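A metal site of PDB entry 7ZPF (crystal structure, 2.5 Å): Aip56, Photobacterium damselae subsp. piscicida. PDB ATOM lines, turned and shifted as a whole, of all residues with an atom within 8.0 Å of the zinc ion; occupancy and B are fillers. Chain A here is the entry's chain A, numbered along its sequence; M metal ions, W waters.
OD2 of Asp 192 sits close to OH of Tyr 223.
ND1 of His 185 sits close to OG1 of Thr 202, 3.1 Å away.
O of Ser 190 sits at hydrogen-bond distance from ND1 of His 185, at 3.2 Å.
NE2 of His 181 lies close to OH of Tyr 223 (3.3 Å).
A ring nitrogen (ND1) of His 181 lies within hydrogen-bond range of the side-chain carboxylate of Glu 203 (3.3 Å).
O of Tyr 223 is in hydrogen-bond range of NH1 of Arg 228 (3.1 Å).
OE1 of Glu 182 lies within hydrogen-bond range of N of Ala 148 (3.3 Å).
Merely in contact with the zinc ion: Tyr 223 and Glu 182.
Five residues have an atom within 4 Å of the zinc ion: His 181, Glu 182, His 185, Asp 192 and Tyr 223.
The zinc ion is bound by OD2 of Asp 192 (2.0 Å).
The zinc ion is bound by a ring nitrogen (NE2) of His 185.
A ring nitrogen (NE2) of His 181 is bound to the zinc ion (2.1 Å).
The zinc ion has three donor atoms within binding distance.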
ATOM      1  N   TYR A 146      -0.957  29.511 -35.948  1.00  0.00           N
ATOM      2  CA  TYR A 146      -2.135  28.709 -35.597  1.00  0.00           C
ATOM      3  C   TYR A 146      -3.178  29.675 -35.064  1.00  0.00           C
ATOM      4  O   TYR A 146      -2.874  30.434 -34.142  1.00  0.00           O
ATOM      5  CB  TYR A 146      -1.797  27.695 -34.503  1.00  0.00           C
ATOM      6  CG  TYR A 146      -1.096  26.440 -34.994  1.00  0.00           C
ATOM      7  CD1 TYR A 146       0.165  26.498 -35.561  1.00  0.00           C
ATOM      8  CD2 TYR A 146      -1.676  25.185 -34.813  1.00  0.00           C
ATOM      9  CE1 TYR A 146       0.830  25.343 -35.951  1.00  0.00           C
ATOM     10  CE2 TYR A 146      -1.015  24.028 -35.194  1.00  0.00           C
ATOM     11  CZ  TYR A 146       0.231  24.114 -35.765  1.00  0.00           C
ATOM     12  OH  TYR A 146       0.879  22.963 -36.129  1.00  0.00           O
ATOM     13  N   GLU A 147      -4.326  29.753 -35.720  1.00  0.00           N
ATOM     14  CA  GLU A 147      -5.300  30.756 -35.395  1.00  0.00           C
ATOM     15  C   GLU A 147      -6.705  30.333 -35.746  1.00  0.00           C
ATOM     16  O   GLU A 147      -6.915  29.765 -36.800  1.00  0.00           O
ATOM     17  CB  GLU A 147      -4.937  31.984 -36.228  1.00  0.00           C
ATOM     18  CG  GLU A 147      -5.545  33.280 -35.731  1.00  0.00           C
ATOM     19  CD  GLU A 147      -5.195  34.467 -36.604  1.00  0.00           C
ATOM     20  OE1 GLU A 147      -4.183  34.382 -37.352  1.00  0.00           O
ATOM     21  OE2 GLU A 147      -5.922  35.492 -36.548  1.00  0.00           O
ATOM     22  N   ALA A 148      -7.662  30.636 -34.875  1.00  0.00           N
ATOM     23  CA  ALA A 148      -9.068  30.379 -35.128  1.00  0.00           C
ATOM     24  C   ALA A 148      -9.572  31.721 -35.597  1.00  0.00           C
ATOM     25  O   ALA A 148      -9.805  32.596 -34.773  1.00  0.00           O
ATOM     26  CB  ALA A 148      -9.751  30.002 -33.850  1.00  0.00           C
ATOM     27  N   ALA A 178      -3.088  20.454 -31.087  1.00  0.00           N
ATOM     28  CA  ALA A 178      -3.025  21.841 -31.519  1.00  0.00           C
ATOM     29  C   ALA A 178      -4.162  22.210 -32.460  1.00  0.00           C
ATOM     30  O   ALA A 178      -4.646  23.344 -32.400  1.00  0.00           O
ATOM     31  CB  ALA A 178      -1.712  22.114 -32.190  1.00  0.00           C
ATOM     32  N   HIS A 181      -7.422  22.187 -30.484  1.00  0.00           N
ATOM     33  CA  HIS A 181      -7.418  23.459 -29.756  1.00  0.00           C
ATOM     34  C   HIS A 181      -8.103  24.599 -30.576  1.00  0.00           C
ATOM     35  O   HIS A 181      -9.107  25.166 -30.112  1.00  0.00           O
ATOM     36  CB  HIS A 181      -5.994  23.830 -29.348  1.00  0.00           C
ATOM     37  CG  HIS A 181      -5.884  25.169 -28.672  1.00  0.00           C
ATOM     38  ND1 HIS A 181      -5.872  25.289 -27.297  1.00  0.00           N
ATOM     39  CD2 HIS A 181      -5.747  26.403 -29.215  1.00  0.00           C
ATOM     40  CE1 HIS A 181      -5.754  26.585 -27.049  1.00  0.00           C
ATOM     41  NE2 HIS A 181      -5.680  27.295 -28.169  1.00  0.00           N
ATOM     42  N   GLU A 182      -7.611  24.876 -31.816  1.00  0.00           N
ATOM     43  CA  GLU A 182      -8.169  25.926 -32.638  1.00  0.00           C
ATOM     44  C   GLU A 182      -9.631  25.692 -33.007  1.00  0.00           C
ATOM     45  O   GLU A 182     -10.382  26.654 -33.157  1.00  0.00           O
ATOM     46  CB  GLU A 182      -7.310  26.207 -33.867  1.00  0.00           C
ATOM     47  CG  GLU A 182      -5.885  26.597 -33.543  1.00  0.00           C
ATOM     48  CD  GLU A 182      -5.615  27.726 -32.563  1.00  0.00           C
ATOM     49  OE1 GLU A 182      -6.353  28.747 -32.576  1.00  0.00           O
ATOM     50  OE2 GLU A 182      -4.615  27.626 -31.815  1.00  0.00           O
ATOM     51  N   ILE A 183     -10.039  24.433 -33.115  1.00  0.00           N
ATOM     52  CA  ILE A 183     -11.448  24.121 -33.395  1.00  0.00           C
ATOM     53  C   ILE A 183     -12.277  24.423 -32.165  1.00  0.00           C
ATOM     54  O   ILE A 183     -13.373  24.955 -32.285  1.00  0.00           O
ATOM     55  CB  ILE A 183     -11.635  22.661 -33.874  1.00  0.00           C
ATOM     56  CG1 ILE A 183     -10.948  22.425 -35.217  1.00  0.00           C
ATOM     57  CG2 ILE A 183     -13.109  22.299 -33.957  1.00  0.00           C
ATOM     58  CD1 ILE A 183     -10.906  21.014 -35.648  1.00  0.00           C
ATOM     59  N   VAL A 184     -11.752  24.148 -30.967  1.00  0.00           N
ATOM     60  CA  VAL A 184     -12.440  24.431 -29.707  1.00  0.00           C
ATOM     61  C   VAL A 184     -12.790  25.920 -29.590  1.00  0.00           C
ATOM     62  O   VAL A 184     -13.877  26.242 -29.154  1.00  0.00           O
ATOM     63  CB  VAL A 184     -11.655  23.869 -28.495  1.00  0.00           C
ATOM     64  CG1 VAL A 184     -12.161  24.438 -27.176  1.00  0.00           C
ATOM     65  CG2 VAL A 184     -11.762  22.356 -28.486  1.00  0.00           C
ATOM     66  N   HIS A 185     -11.964  26.790 -30.102  1.00  0.00           N
ATOM     67  CA  HIS A 185     -12.206  28.228 -30.121  1.00  0.00           C
ATOM     68  C   HIS A 185     -13.435  28.593 -30.958  1.00  0.00           C
ATOM     69  O   HIS A 185     -14.018  29.642 -30.748  1.00  0.00           O
ATOM     70  CB  HIS A 185     -10.991  28.932 -30.754  1.00  0.00           C
ATOM     71  CG  HIS A 185      -9.845  29.218 -29.847  1.00  0.00           C
ATOM     72  ND1 HIS A 185     -10.026  29.548 -28.530  1.00  0.00           N
ATOM     73  CD2 HIS A 185      -8.536  29.353 -30.155  1.00  0.00           C
ATOM     74  CE1 HIS A 185      -8.814  29.766 -28.043  1.00  0.00           C
ATOM     75  NE2 HIS A 185      -7.874  29.677 -28.978  1.00  0.00           N
ATOM     76  N   SER A 190     -14.758  29.917 -26.527  1.00  0.00           N
ATOM     77  CA  SER A 190     -13.809  30.125 -25.454  1.00  0.00           C
ATOM     78  C   SER A 190     -12.626  30.912 -25.954  1.00  0.00           C
ATOM     79  O   SER A 190     -12.426  31.089 -27.152  1.00  0.00           O
ATOM     80  CB  SER A 190     -13.356  28.774 -24.888  1.00  0.00           C
ATOM     81  OG  SER A 190     -12.623  28.004 -25.824  1.00  0.00           O
ATOM     82  N   SER A 191     -11.890  31.459 -25.023  1.00  0.00           N
ATOM     83  CA  SER A 191     -10.711  32.241 -25.257  1.00  0.00           C
ATOM     84  C   SER A 191      -9.521  31.582 -24.553  1.00  0.00           C
ATOM     85  O   SER A 191      -9.648  30.483 -23.996  1.00  0.00           O
ATOM     86  CB  SER A 191     -10.936  33.663 -24.744  1.00  0.00           C
ATOM     87  OG  SER A 191     -11.512  34.466 -25.762  1.00  0.00           O
ATOM     88  N   ASP A 192      -8.372  32.206 -24.628  1.00  0.00           N
ATOM     89  CA  ASP A 192      -7.194  31.723 -23.937  1.00  0.00           C
ATOM     90  C   ASP A 192      -6.831  32.711 -22.825  1.00  0.00           C
ATOM     91  O   ASP A 192      -7.459  33.775 -22.696  1.00  0.00           O
ATOM     92  CB  ASP A 192      -6.064  31.516 -24.938  1.00  0.00           C
ATOM     93  CG  ASP A 192      -6.072  30.124 -25.515  1.00  0.00           C
ATOM     94  OD1 ASP A 192      -6.435  29.176 -24.779  1.00  0.00           O
ATOM     95  OD2 ASP A 192      -5.696  29.979 -26.713  1.00  0.00           O
ATOM     96  N   THR A 193      -5.859  32.343 -21.989  1.00  0.00           N
ATOM     97  CA  THR A 193      -5.437  33.230 -20.916  1.00  0.00           C
ATOM     98  C   THR A 193      -3.960  33.493 -20.968  1.00  0.00           C
ATOM     99  O   THR A 193      -3.142  32.630 -21.321  1.00  0.00           O
ATOM    100  CB  THR A 193      -5.935  32.783 -19.541  1.00  0.00           C
ATOM    101  OG1 THR A 193      -5.919  33.913 -18.647  1.00  0.00           O
ATOM    102  CG2 THR A 193      -5.132  31.635 -18.987  1.00  0.00           C
ATOM    103  N   GLN A 199      -3.623  27.403 -17.879  1.00  0.00           N
ATOM    104  CA  GLN A 199      -3.730  26.871 -19.245  1.00  0.00           C
ATOM    105  C   GLN A 199      -4.834  27.576 -20.042  1.00  0.00           C
ATOM    106  O   GLN A 199      -4.702  27.734 -21.256  1.00  0.00           O
ATOM    107  CB  GLN A 199      -3.996  25.340 -19.234  1.00  0.00           C
ATOM    108  CG  GLN A 199      -3.016  24.518 -18.396  1.00  0.00           C
ATOM    109  CD  GLN A 199      -1.745  24.102 -19.123  1.00  0.00           C
ATOM    110  OE1 GLN A 199      -0.892  24.916 -19.479  1.00  0.00           O
ATOM    111  NE2 GLN A 199      -1.572  22.797 -19.336  1.00  0.00           N
ATOM    112  N   THR A 202      -9.644  26.826 -23.331  1.00  0.00           N
ATOM    113  CA  THR A 202      -9.513  26.151 -24.628  1.00  0.00           C
ATOM    114  C   THR A 202      -8.465  25.070 -24.524  1.00  0.00           C
ATOM    115  O   THR A 202      -8.707  23.944 -24.945  1.00  0.00           O
ATOM    116  CB  THR A 202      -9.192  27.161 -25.718  1.00  0.00           C
ATOM    117  OG1 THR A 202     -10.161  28.206 -25.688  1.00  0.00           O
ATOM    118  CG2 THR A 202      -9.138  26.527 -27.096  1.00  0.00           C
ATOM    119  N   GLU A 203      -7.307  25.392 -23.910  1.00  0.00           N
ATOM    120  CA  GLU A 203      -6.220  24.437 -23.728  1.00  0.00           C
ATOM    121  C   GLU A 203      -6.657  23.284 -22.788  1.00  0.00           C
ATOM    122  O   GLU A 203      -6.301  22.135 -23.027  1.00  0.00           O
ATOM    123  CB  GLU A 203      -4.959  25.148 -23.217  1.00  0.00           C
ATOM    124  CG  GLU A 203      -3.638  24.466 -23.505  1.00  0.00           C
ATOM    125  CD  GLU A 203      -3.532  23.676 -24.799  1.00  0.00           C
ATOM    126  OE1 GLU A 203      -3.840  22.453 -24.760  1.00  0.00           O
ATOM    127  OE2 GLU A 203      -3.152  24.241 -25.846  1.00  0.00           O
ATOM    128  N   TYR A 223      -0.482  28.711 -20.331  1.00  0.00           N
ATOM    129  CA  TYR A 223      -0.616  28.932 -21.770  1.00  0.00           C
ATOM    130  C   TYR A 223       0.489  29.836 -22.302  1.00  0.00           C
ATOM    131  O   TYR A 223       0.985  29.611 -23.406  1.00  0.00           O
ATOM    132  CB  TYR A 223      -2.013  29.428 -22.168  1.00  0.00           C
ATOM    133  CG  TYR A 223      -2.276  29.259 -23.653  1.00  0.00           C
ATOM    134  CD1 TYR A 223      -2.618  28.025 -24.174  1.00  0.00           C
ATOM    135  CD2 TYR A 223      -2.084  30.307 -24.532  1.00  0.00           C
ATOM    136  CE1 TYR A 223      -2.810  27.849 -25.547  1.00  0.00           C
ATOM    137  CE2 TYR A 223      -2.253  30.140 -25.906  1.00  0.00           C
ATOM    138  CZ  TYR A 223      -2.613  28.910 -26.402  1.00  0.00           C
ATOM    139  OH  TYR A 223      -2.783  28.749 -27.754  1.00  0.00           O
ATOM    140  N   ARG A 228       6.870  26.680 -23.068  1.00  0.00           N
ATOM    141  CA  ARG A 228       5.808  26.192 -23.948  1.00  0.00           C
ATOM    142  C   ARG A 228       5.942  26.820 -25.330  1.00  0.00           C
ATOM    143  O   ARG A 228       5.938  26.100 -26.328  1.00  0.00           O
ATOM    144  CB  ARG A 228       4.426  26.522 -23.355  1.00  0.00           C
ATOM    145  CG  ARG A 228       3.300  25.964 -24.199  1.00  0.00           C
ATOM    146  CD  ARG A 228       1.920  26.298 -23.692  1.00  0.00           C
ATOM    147  NE  ARG A 228       0.919  25.746 -24.606  1.00  0.00           N
ATOM    148  CZ  ARG A 228       0.376  26.408 -25.611  1.00  0.00           C
ATOM    149  NH1 ARG A 228       0.675  27.681 -25.832  1.00  0.00           N
ATOM    150  NH2 ARG A 228      -0.480  25.804 -26.420  1.00  0.00           N
HETATM  151 ZN    ZN M   1      -5.910  29.308 -28.613  1.00  0.00          ZN
HETATM  152  O   HOH W   1      -4.395  31.705 -30.552  1.00  0.00           O
